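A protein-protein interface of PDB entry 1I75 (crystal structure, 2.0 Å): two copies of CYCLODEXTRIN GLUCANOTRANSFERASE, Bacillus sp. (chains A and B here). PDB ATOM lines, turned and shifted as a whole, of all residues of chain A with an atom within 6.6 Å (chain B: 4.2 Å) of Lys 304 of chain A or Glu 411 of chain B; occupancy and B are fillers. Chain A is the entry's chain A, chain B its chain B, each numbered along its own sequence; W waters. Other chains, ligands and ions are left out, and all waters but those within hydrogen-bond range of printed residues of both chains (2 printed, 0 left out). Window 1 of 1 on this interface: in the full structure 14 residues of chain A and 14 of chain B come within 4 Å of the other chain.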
ATOM      1  N   LYS A 288     -10.794 -11.864   2.293  1.00  0.00           N
ATOM      2  CA  LYS A 288     -10.563 -10.445   2.057  1.00  0.00           C
ATOM      3  C   LYS A 288     -10.332  -9.714   3.377  1.00  0.00           C
ATOM      4  O   LYS A 288      -9.442  -8.845   3.454  1.00  0.00           O
ATOM      5  CB  LYS A 288     -11.773  -9.839   1.294  1.00  0.00           C
ATOM      6  CG  LYS A 288     -11.607  -8.350   0.899  1.00  0.00           C
ATOM      7  CD  LYS A 288     -10.385  -8.093   0.003  1.00  0.00           C
ATOM      8  CE  LYS A 288     -10.522  -8.889  -1.301  1.00  0.00           C
ATOM      9  NZ  LYS A 288      -9.320  -8.787  -2.117  1.00  0.00           N
ATOM     10  N   ASN A 299      -6.422  -3.187   0.375  1.00  0.00           N
ATOM     11  CA  ASN A 299      -6.850  -2.054   1.165  1.00  0.00           C
ATOM     12  C   ASN A 299      -8.355  -1.904   1.229  1.00  0.00           C
ATOM     13  O   ASN A 299      -9.102  -2.783   0.773  1.00  0.00           O
ATOM     14  CB  ASN A 299      -6.209  -0.799   0.596  1.00  0.00           C
ATOM     15  CG  ASN A 299      -6.555  -0.421  -0.825  1.00  0.00           C
ATOM     16  OD1 ASN A 299      -7.616  -0.693  -1.391  1.00  0.00           O
ATOM     17  ND2 ASN A 299      -5.581   0.214  -1.446  1.00  0.00           N
ATOM     18  N   MET A 300      -8.859  -0.774   1.733  1.00  0.00           N
ATOM     19  CA  MET A 300     -10.287  -0.636   1.961  1.00  0.00           C
ATOM     20  C   MET A 300     -11.215  -0.717   0.769  1.00  0.00           C
ATOM     21  O   MET A 300     -12.386  -1.089   0.902  1.00  0.00           O
ATOM     22  CB  MET A 300     -10.530   0.669   2.719  1.00  0.00           C
ATOM     23  CG  MET A 300     -10.015   0.581   4.161  1.00  0.00           C
ATOM     24  SD  MET A 300     -10.732  -0.810   5.083  1.00  0.00           S
ATOM     25  CE  MET A 300      -9.951  -0.480   6.632  1.00  0.00           C
ATOM     26  N   TYR A 301     -10.686  -0.423  -0.416  1.00  0.00           N
ATOM     27  CA  TYR A 301     -11.440  -0.546  -1.663  1.00  0.00           C
ATOM     28  C   TYR A 301     -11.713  -2.009  -2.000  1.00  0.00           C
ATOM     29  O   TYR A 301     -12.800  -2.350  -2.489  1.00  0.00           O
ATOM     30  CB  TYR A 301     -10.662   0.127  -2.791  1.00  0.00           C
ATOM     31  CG  TYR A 301     -10.844   1.638  -2.706  1.00  0.00           C
ATOM     32  CD1 TYR A 301      -9.812   2.483  -2.288  1.00  0.00           C
ATOM     33  CD2 TYR A 301     -12.096   2.155  -3.035  1.00  0.00           C
ATOM     34  CE1 TYR A 301     -10.046   3.858  -2.187  1.00  0.00           C
ATOM     35  CE2 TYR A 301     -12.334   3.510  -2.938  1.00  0.00           C
ATOM     36  CZ  TYR A 301     -11.313   4.346  -2.525  1.00  0.00           C
ATOM     37  OH  TYR A 301     -11.613   5.677  -2.489  1.00  0.00           O
ATOM     38  N   GLY A 302     -10.762  -2.902  -1.658  1.00  0.00           N
ATOM     39  CA  GLY A 302     -10.982  -4.330  -1.824  1.00  0.00           C
ATOM     40  C   GLY A 302     -12.065  -4.815  -0.868  1.00  0.00           C
ATOM     41  O   GLY A 302     -12.914  -5.627  -1.218  1.00  0.00           O
ATOM     42  N   LEU A 303     -12.073  -4.332   0.368  1.00  0.00           N
ATOM     43  CA  LEU A 303     -13.092  -4.684   1.350  1.00  0.00           C
ATOM     44  C   LEU A 303     -14.470  -4.233   0.886  1.00  0.00           C
ATOM     45  O   LEU A 303     -15.431  -5.000   0.903  1.00  0.00           O
ATOM     46  CB  LEU A 303     -12.761  -4.020   2.678  1.00  0.00           C
ATOM     47  CG  LEU A 303     -13.452  -4.550   3.936  1.00  0.00           C
ATOM     48  CD1 LEU A 303     -12.811  -5.861   4.370  1.00  0.00           C
ATOM     49  CD2 LEU A 303     -13.279  -3.542   5.057  1.00  0.00           C
ATOM     50  N   LYS A 304     -14.585  -2.973   0.455  1.00  0.00           N
ATOM     51  CA  LYS A 304     -15.792  -2.385  -0.125  1.00  0.00           C
ATOM     52  C   LYS A 304     -16.272  -3.239  -1.283  1.00  0.00           C
ATOM     53  O   LYS A 304     -17.430  -3.641  -1.295  1.00  0.00           O
ATOM     54  CB  LYS A 304     -15.469  -0.976  -0.618  1.00  0.00           C
ATOM     55  CG  LYS A 304     -16.528  -0.253  -1.462  1.00  0.00           C
ATOM     56  CD  LYS A 304     -15.980   1.094  -1.909  1.00  0.00           C
ATOM     57  CE  LYS A 304     -16.731   1.588  -3.134  1.00  0.00           C
ATOM     58  NZ  LYS A 304     -18.101   1.917  -2.781  1.00  0.00           N
ATOM     59  N   ALA A 305     -15.394  -3.590  -2.226  1.00  0.00           N
ATOM     60  CA  ALA A 305     -15.810  -4.367  -3.387  1.00  0.00           C
ATOM     61  C   ALA A 305     -16.297  -5.761  -3.008  1.00  0.00           C
ATOM     62  O   ALA A 305     -17.242  -6.270  -3.622  1.00  0.00           O
ATOM     63  CB  ALA A 305     -14.647  -4.486  -4.361  1.00  0.00           C
ATOM     64  N   MET A 306     -15.711  -6.398  -1.986  1.00  0.00           N
ATOM     65  CA  MET A 306     -16.192  -7.693  -1.517  1.00  0.00           C
ATOM     66  C   MET A 306     -17.574  -7.556  -0.874  1.00  0.00           C
ATOM     67  O   MET A 306     -18.469  -8.360  -1.145  1.00  0.00           O
ATOM     68  CB  MET A 306     -15.169  -8.286  -0.505  1.00  0.00           C
ATOM     69  CG  MET A 306     -15.525  -9.604   0.217  1.00  0.00           C
ATOM     70  SD  MET A 306     -16.696  -9.380   1.583  1.00  0.00           S
ATOM     71  CE  MET A 306     -15.552  -8.503   2.622  1.00  0.00           C
ATOM     72  N   LEU A 307     -17.807  -6.527  -0.058  1.00  0.00           N
ATOM     73  CA  LEU A 307     -19.097  -6.369   0.596  1.00  0.00           C
ATOM     74  C   LEU A 307     -20.146  -6.057  -0.462  1.00  0.00           C
ATOM     75  O   LEU A 307     -21.244  -6.603  -0.459  1.00  0.00           O
ATOM     76  CB  LEU A 307     -18.966  -5.237   1.632  1.00  0.00           C
ATOM     77  CG  LEU A 307     -18.090  -5.493   2.856  1.00  0.00           C
ATOM     78  CD1 LEU A 307     -17.755  -4.196   3.589  1.00  0.00           C
ATOM     79  CD2 LEU A 307     -18.830  -6.418   3.765  1.00  0.00           C
ATOM     80  N   GLU A 308     -19.793  -5.236  -1.452  1.00  0.00           N
ATOM     81  CA  GLU A 308     -20.754  -4.839  -2.468  1.00  0.00           C
ATOM     82  C   GLU A 308     -21.078  -5.957  -3.433  1.00  0.00           C
ATOM     83  O   GLU A 308     -22.246  -6.194  -3.779  1.00  0.00           O
ATOM     84  CB  GLU A 308     -20.221  -3.623  -3.210  1.00  0.00           C
ATOM     85  CG  GLU A 308     -20.384  -2.396  -2.296  1.00  0.00           C
ATOM     86  CD  GLU A 308     -19.812  -1.061  -2.772  1.00  0.00           C
ATOM     87  OE1 GLU A 308     -20.049  -0.067  -2.074  1.00  0.00           O
ATOM     88  OE2 GLU A 308     -19.116  -1.000  -3.800  1.00  0.00           O
ATOM     89  N   GLY A 309     -20.042  -6.692  -3.800  1.00  0.00           N
ATOM     90  CA  GLY A 309     -20.174  -7.823  -4.697  1.00  0.00           C
ATOM     91  C   GLY A 309     -20.864  -9.000  -4.044  1.00  0.00           C
ATOM     92  O   GLY A 309     -21.780  -9.577  -4.642  1.00  0.00           O
ATOM     93  N   GLU A 411     -21.472   1.932   2.093  1.00  0.00           N
ATOM     94  CA  GLU A 411     -20.251   2.619   2.408  1.00  0.00           C
ATOM     95  C   GLU A 411     -20.548   4.120   2.390  1.00  0.00           C
ATOM     96  O   GLU A 411     -21.077   4.637   1.406  1.00  0.00           O
ATOM     97  CB  GLU A 411     -19.206   2.171   1.385  1.00  0.00           C
ATOM     98  CG  GLU A 411     -17.882   2.941   1.430  1.00  0.00           C
ATOM     99  CD  GLU A 411     -17.845   4.127   0.453  1.00  0.00           C
ATOM    100  OE1 GLU A 411     -17.827   3.930  -0.753  1.00  0.00           O
ATOM    101  OE2 GLU A 411     -17.833   5.266   0.884  1.00  0.00           O
ATOM    102  N   ARG A 412     -20.261   4.820   3.496  1.00  0.00           N
ATOM    103  CA  ARG A 412     -20.494   6.255   3.654  1.00  0.00           C
ATOM    104  C   ARG A 412     -19.234   7.102   3.539  1.00  0.00           C
ATOM    105  O   ARG A 412     -19.295   8.269   3.160  1.00  0.00           O
ATOM    106  CB  ARG A 412     -21.138   6.524   5.007  1.00  0.00           C
ATOM    107  CG  ARG A 412     -22.550   5.986   5.132  1.00  0.00           C
ATOM    108  CD  ARG A 412     -23.480   6.708   4.176  1.00  0.00           C
ATOM    109  NE  ARG A 412     -24.853   6.610   4.638  1.00  0.00           N
ATOM    110  CZ  ARG A 412     -25.836   7.402   4.166  1.00  0.00           C
ATOM    111  NH1 ARG A 412     -25.629   8.325   3.221  1.00  0.00           N
ATOM    112  NH2 ARG A 412     -27.059   7.301   4.675  1.00  0.00           N
ATOM    113  N   TRP A 413     -18.046   6.568   3.820  1.00  0.00           N
ATOM    114  CA  TRP A 413     -16.797   7.295   3.680  1.00  0.00           C
ATOM    115  C   TRP A 413     -15.729   6.236   3.483  1.00  0.00           C
ATOM    116  O   TRP A 413     -15.846   5.137   4.060  1.00  0.00           O
ATOM    117  CB  TRP A 413     -16.481   8.112   4.952  1.00  0.00           C
ATOM    118  CG  TRP A 413     -15.557   9.306   4.739  1.00  0.00           C
ATOM    119  CD1 TRP A 413     -16.072  10.558   4.486  1.00  0.00           C
ATOM    120  CD2 TRP A 413     -14.178   9.307   4.774  1.00  0.00           C
ATOM    121  NE1 TRP A 413     -15.021  11.351   4.364  1.00  0.00           N
ATOM    122  CE2 TRP A 413     -13.880  10.654   4.526  1.00  0.00           C
ATOM    123  CE3 TRP A 413     -13.164   8.379   4.980  1.00  0.00           C
ATOM    124  CZ2 TRP A 413     -12.546  11.075   4.482  1.00  0.00           C
ATOM    125  CZ3 TRP A 413     -11.823   8.802   4.932  1.00  0.00           C
ATOM    126  CH2 TRP A 413     -11.512  10.143   4.686  1.00  0.00           C
ATOM    127  N   ILE A 414     -14.688   6.541   2.707  1.00  0.00           N
ATOM    128  CA  ILE A 414     -13.623   5.588   2.473  1.00  0.00           C
ATOM    129  C   ILE A 414     -12.385   6.268   1.975  1.00  0.00           C
ATOM    130  O   ILE A 414     -12.431   7.367   1.419  1.00  0.00           O
ATOM    131  CB  ILE A 414     -14.084   4.496   1.436  1.00  0.00           C
ATOM    132  CG1 ILE A 414     -13.060   3.383   1.306  1.00  0.00           C
ATOM    133  CG2 ILE A 414     -14.339   5.164   0.099  1.00  0.00           C
ATOM    134  CD1 ILE A 414     -13.708   2.102   0.838  1.00  0.00           C
ATOM    135  N   ILE A 419     -12.674   2.904   6.460  1.00  0.00           N
ATOM    136  CA  ILE A 419     -13.986   2.704   5.894  1.00  0.00           C
ATOM    137  C   ILE A 419     -15.001   3.108   6.961  1.00  0.00           C
ATOM    138  O   ILE A 419     -14.746   2.961   8.169  1.00  0.00           O
ATOM    139  CB  ILE A 419     -14.150   1.222   5.446  1.00  0.00           C
ATOM    140  CG1 ILE A 419     -15.376   1.184   4.530  1.00  0.00           C
ATOM    141  CG2 ILE A 419     -14.251   0.256   6.620  1.00  0.00           C
ATOM    142  CD1 ILE A 419     -15.615  -0.155   3.819  1.00  0.00           C
ATOM    143  N   LYS B 304     -21.363  12.889  -3.621  1.00  0.00           N
ATOM    144  CA  LYS B 304     -21.744  11.519  -3.261  1.00  0.00           C
ATOM    145  C   LYS B 304     -22.980  11.543  -2.366  1.00  0.00           C
ATOM    146  O   LYS B 304     -23.955  10.849  -2.665  1.00  0.00           O
ATOM    147  CB  LYS B 304     -20.604  10.819  -2.496  1.00  0.00           C
ATOM    148  CG  LYS B 304     -20.941   9.428  -1.934  1.00  0.00           C
ATOM    149  CD  LYS B 304     -19.752   8.927  -1.107  1.00  0.00           C
ATOM    150  CE  LYS B 304     -20.148   7.834  -0.140  1.00  0.00           C
ATOM    151  NZ  LYS B 304     -20.616   6.619  -0.796  1.00  0.00           N
ATOM    152  N   GLU B 308     -26.603   9.844  -3.450  1.00  0.00           N
ATOM    153  CA  GLU B 308     -27.143   8.768  -2.648  1.00  0.00           C
ATOM    154  C   GLU B 308     -28.406   9.155  -1.897  1.00  0.00           C
ATOM    155  O   GLU B 308     -29.304   8.322  -1.769  1.00  0.00           O
ATOM    156  CB  GLU B 308     -26.062   8.289  -1.677  1.00  0.00           C
ATOM    157  CG  GLU B 308     -25.078   7.385  -2.421  1.00  0.00           C
ATOM    158  CD  GLU B 308     -23.759   7.104  -1.723  1.00  0.00           C
ATOM    159  OE1 GLU B 308     -22.865   6.578  -2.389  1.00  0.00           O
ATOM    160  OE2 GLU B 308     -23.608   7.420  -0.538  1.00  0.00           O
ATOM    161  N   HIS B 410     -23.711   4.321  -8.537  1.00  0.00           N
ATOM    162  CA  HIS B 410     -22.934   3.605  -7.539  1.00  0.00           C
ATOM    163  C   HIS B 410     -21.564   4.219  -7.442  1.00  0.00           C
ATOM    164  O   HIS B 410     -20.847   4.163  -8.439  1.00  0.00           O
ATOM    165  CB  HIS B 410     -22.964   2.142  -8.028  1.00  0.00           C
ATOM    166  CG  HIS B 410     -22.149   1.069  -7.316  1.00  0.00           C
ATOM    167  ND1 HIS B 410     -21.908  -0.173  -7.773  1.00  0.00           N
ATOM    168  CD2 HIS B 410     -21.551   1.163  -6.074  1.00  0.00           C
ATOM    169  CE1 HIS B 410     -21.208  -0.816  -6.863  1.00  0.00           C
ATOM    170  NE2 HIS B 410     -21.003  -0.006  -5.858  1.00  0.00           N
ATOM    171  N   GLU B 411     -21.139   4.827  -6.329  1.00  0.00           N
ATOM    172  CA  GLU B 411     -19.795   5.365  -6.233  1.00  0.00           C
ATOM    173  C   GLU B 411     -18.867   4.166  -6.066  1.00  0.00           C
ATOM    174  O   GLU B 411     -19.148   3.252  -5.278  1.00  0.00           O
ATOM    175  CB  GLU B 411     -19.709   6.318  -5.039  1.00  0.00           C
ATOM    176  CG  GLU B 411     -18.312   6.802  -4.623  1.00  0.00           C
ATOM    177  CD  GLU B 411     -17.751   5.928  -3.502  1.00  0.00           C
ATOM    178  OE1 GLU B 411     -18.310   5.948  -2.416  1.00  0.00           O
ATOM    179  OE2 GLU B 411     -16.778   5.204  -3.706  1.00  0.00           O
ATOM    180  N   ARG B 412     -17.791   4.153  -6.843  1.00  0.00           N
ATOM    181  CA  ARG B 412     -16.846   3.049  -6.821  1.00  0.00           C
ATOM    182  C   ARG B 412     -15.508   3.597  -6.410  1.00  0.00           C
ATOM    183  O   ARG B 412     -14.707   2.838  -5.871  1.00  0.00           O
ATOM    184  CB  ARG B 412     -16.695   2.408  -8.185  1.00  0.00           C
ATOM    185  CG  ARG B 412     -17.934   1.784  -8.797  1.00  0.00           C
ATOM    186  CD  ARG B 412     -18.175   0.558  -8.019  1.00  0.00           C
ATOM    187  NE  ARG B 412     -18.852  -0.444  -8.808  1.00  0.00           N
ATOM    188  CZ  ARG B 412     -18.594  -1.760  -8.636  1.00  0.00           C
ATOM    189  NH1 ARG B 412     -17.712  -2.194  -7.742  1.00  0.00           N
ATOM    190  NH2 ARG B 412     -19.241  -2.694  -9.343  1.00  0.00           N
ATOM    191  N   TRP B 413     -15.155   4.865  -6.566  1.00  0.00           N
ATOM    192  CA  TRP B 413     -13.856   5.319  -6.077  1.00  0.00           C
ATOM    193  C   TRP B 413     -14.036   6.772  -5.725  1.00  0.00           C
ATOM    194  O   TRP B 413     -14.766   7.466  -6.461  1.00  0.00           O
ATOM    195  CB  TRP B 413     -12.775   5.192  -7.146  1.00  0.00           C
ATOM    196  CG  TRP B 413     -11.375   5.186  -6.557  1.00  0.00           C
ATOM    197  CD1 TRP B 413     -10.780   3.988  -6.215  1.00  0.00           C
ATOM    198  CD2 TRP B 413     -10.567   6.286  -6.313  1.00  0.00           C
ATOM    199  NE1 TRP B 413      -9.589   4.331  -5.754  1.00  0.00           N
ATOM    200  CE2 TRP B 413      -9.413   5.678  -5.795  1.00  0.00           C
ATOM    201  CE3 TRP B 413     -10.631   7.681  -6.446  1.00  0.00           C
ATOM    202  CZ2 TRP B 413      -8.315   6.463  -5.407  1.00  0.00           C
ATOM    203  CZ3 TRP B 413      -9.531   8.467  -6.054  1.00  0.00           C
ATOM    204  CH2 TRP B 413      -8.375   7.859  -5.538  1.00  0.00           C
ATOM    205  N   ILE B 414     -13.452   7.275  -4.636  1.00  0.00           N
ATOM    206  CA  ILE B 414     -13.643   8.659  -4.275  1.00  0.00           C
ATOM    207  C   ILE B 414     -12.521   9.130  -3.357  1.00  0.00           C
ATOM    208  O   ILE B 414     -11.850   8.350  -2.686  1.00  0.00           O
ATOM    209  CB  ILE B 414     -15.069   8.814  -3.589  1.00  0.00           C
ATOM    210  CG1 ILE B 414     -15.451  10.298  -3.441  1.00  0.00           C
ATOM    211  CG2 ILE B 414     -15.073   8.091  -2.239  1.00  0.00           C
ATOM    212  CD1 ILE B 414     -16.875  10.524  -2.930  1.00  0.00           C
ATOM    213  N   ILE B 420     -15.534   8.557  -9.133  1.00  0.00           N
ATOM    214  CA  ILE B 420     -15.711   7.609 -10.201  1.00  0.00           C
ATOM    215  C   ILE B 420     -16.966   6.863  -9.784  1.00  0.00           C
ATOM    216  O   ILE B 420     -17.002   6.211  -8.730  1.00  0.00           O
ATOM    217  CB  ILE B 420     -14.513   6.629 -10.308  1.00  0.00           C
ATOM    218  CG1 ILE B 420     -13.202   7.397 -10.586  1.00  0.00           C
ATOM    219  CG2 ILE B 420     -14.793   5.626 -11.444  1.00  0.00           C
ATOM    220  CD1 ILE B 420     -11.898   6.562 -10.658  1.00  0.00           C
HETATM  221  O   HOH W   1     -16.992  -1.769  -5.253  1.00  0.00           O
HETATM  222  O   HOH W   2     -23.741   9.518   1.507  1.00  0.00           O
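Water W1 bridges the guanidinium group of Arg 412 of chain B (2.6 Å) and the side-chain carboxylate of Glu 308 of chain A (2.7 Å). Water W2 bridges the guanidinium group (NH1) of Arg 412 of chain A and the side-chain carboxylate (OE2) of Glu 308 of chain B.
Lys 304 of chain A touches Glu 411 of chain B, and with the chains exchanged Glu 411 of chain A touches Lys 304 of chain B. Lys 304 of chain A touches Arg 412 of chain B, and with the chains exchanged Arg 412 of chain A touches Lys 304 of chain B. Glu 411 of chain A touches its own counterpart, Glu 411 of chain B. Ile 414 of chain B touches its own counterpart, Ile 414 of chain A. Of the 10 pairs that touch across the chains among the printed residues, 6 have their exchanged pair printed and touching as well.
The backbone carbonyl oxygen (O) of Ile 414 of chain B is in hydrogen-bond range of the side-chain hydroxyl (OH) of Tyr 301 of chain A (2.7 Å). OE2 of Glu 411 of chain B is in salt-bridge range of NZ of Lys 304 of chain A, at 3.7 Å. The side-chain carboxylate of Glu 308 of chain A sits at hydrogen-bond distance from a ring nitrogen (NE2) of His 410 of chain B. The side-chain amino group (NZ) of Lys 304 of chain B is in salt-bridge range of the side-chain carboxylate (OE2) of Glu 411 of chain A (3.5 Å). The side-chain carboxylate (OE1) of Glu 411 of chain A lies close to the side-chain carboxylate (OE1) of Glu 411 of chain B, at 2.7 Å.
CE2 of Tyr 301 of chain A touches O of Arg 412 of chain B (3.8 Å). Tyr 301 of chain A touches Trp 413 of chain B (CE1 to NE1, 3.6 Å). O of Arg 412 of chain B touches CE of Lys 304 of chain A, at 3.6 Å. Lys 304 of chain B touches Arg 412 of chain A (CE to O, 3.4 Å). Ile 414 of chain A touches Ile 414 of chain B.
Among the printed residues, Asp or Glu carboxylates within 4 Å of a Lys or Arg side-chain nitrogen of the other chain: Lys 304 of chain A with Glu 411 of chain B (3.7 Å) and Glu 411 of chain A with Lys 304 of chain B (3.5 Å).
Of the printed residues of chain A, His 410 of chain B touches Glu 308 (3.0 Å). Of the printed residues of chain A, Arg 412 of chain B touches Tyr 301 and Lys 304. Of the printed residues of chain A, Trp 413 of chain B touches Tyr 301 (3.6 Å). Of the printed residues of chain A, Ile 414 of chain B touches Tyr 301 and Ile 414. The nearest printed residue of chain A that does not touch Glu 411 of chain B is Glu 308 of chain A (4.5 Å). The nearest printed residue of chain B that does not touch Ile 414 of chain A is Glu 411 of chain B (4.5 Å).
OE1 of Glu 308 of chain A lies within salt-bridge range of NZ of Lys 304 of chain A (2.9 Å). The side-chain carboxylate of Glu 308 of chain B is in salt-bridge range of the side-chain amino group of Lys 304 of chain B (2.8 Å). NE of Arg 412 of chain B sits close to ND1 of His 410 of chain B (3.2 Å). OE2 of Glu 411 of chain B is in hydrogen-bond range of N of Trp 413 of chain B. The backbone NH of Arg 412 of chain B lies within hydrogen-bond range of the backbone carbonyl oxygen of Ile 420 of chain B, at 2.9 Å. O of Trp 413 of chain B is in hydrogen-bond range of N of Ile 420 of chain B (3.0 Å).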
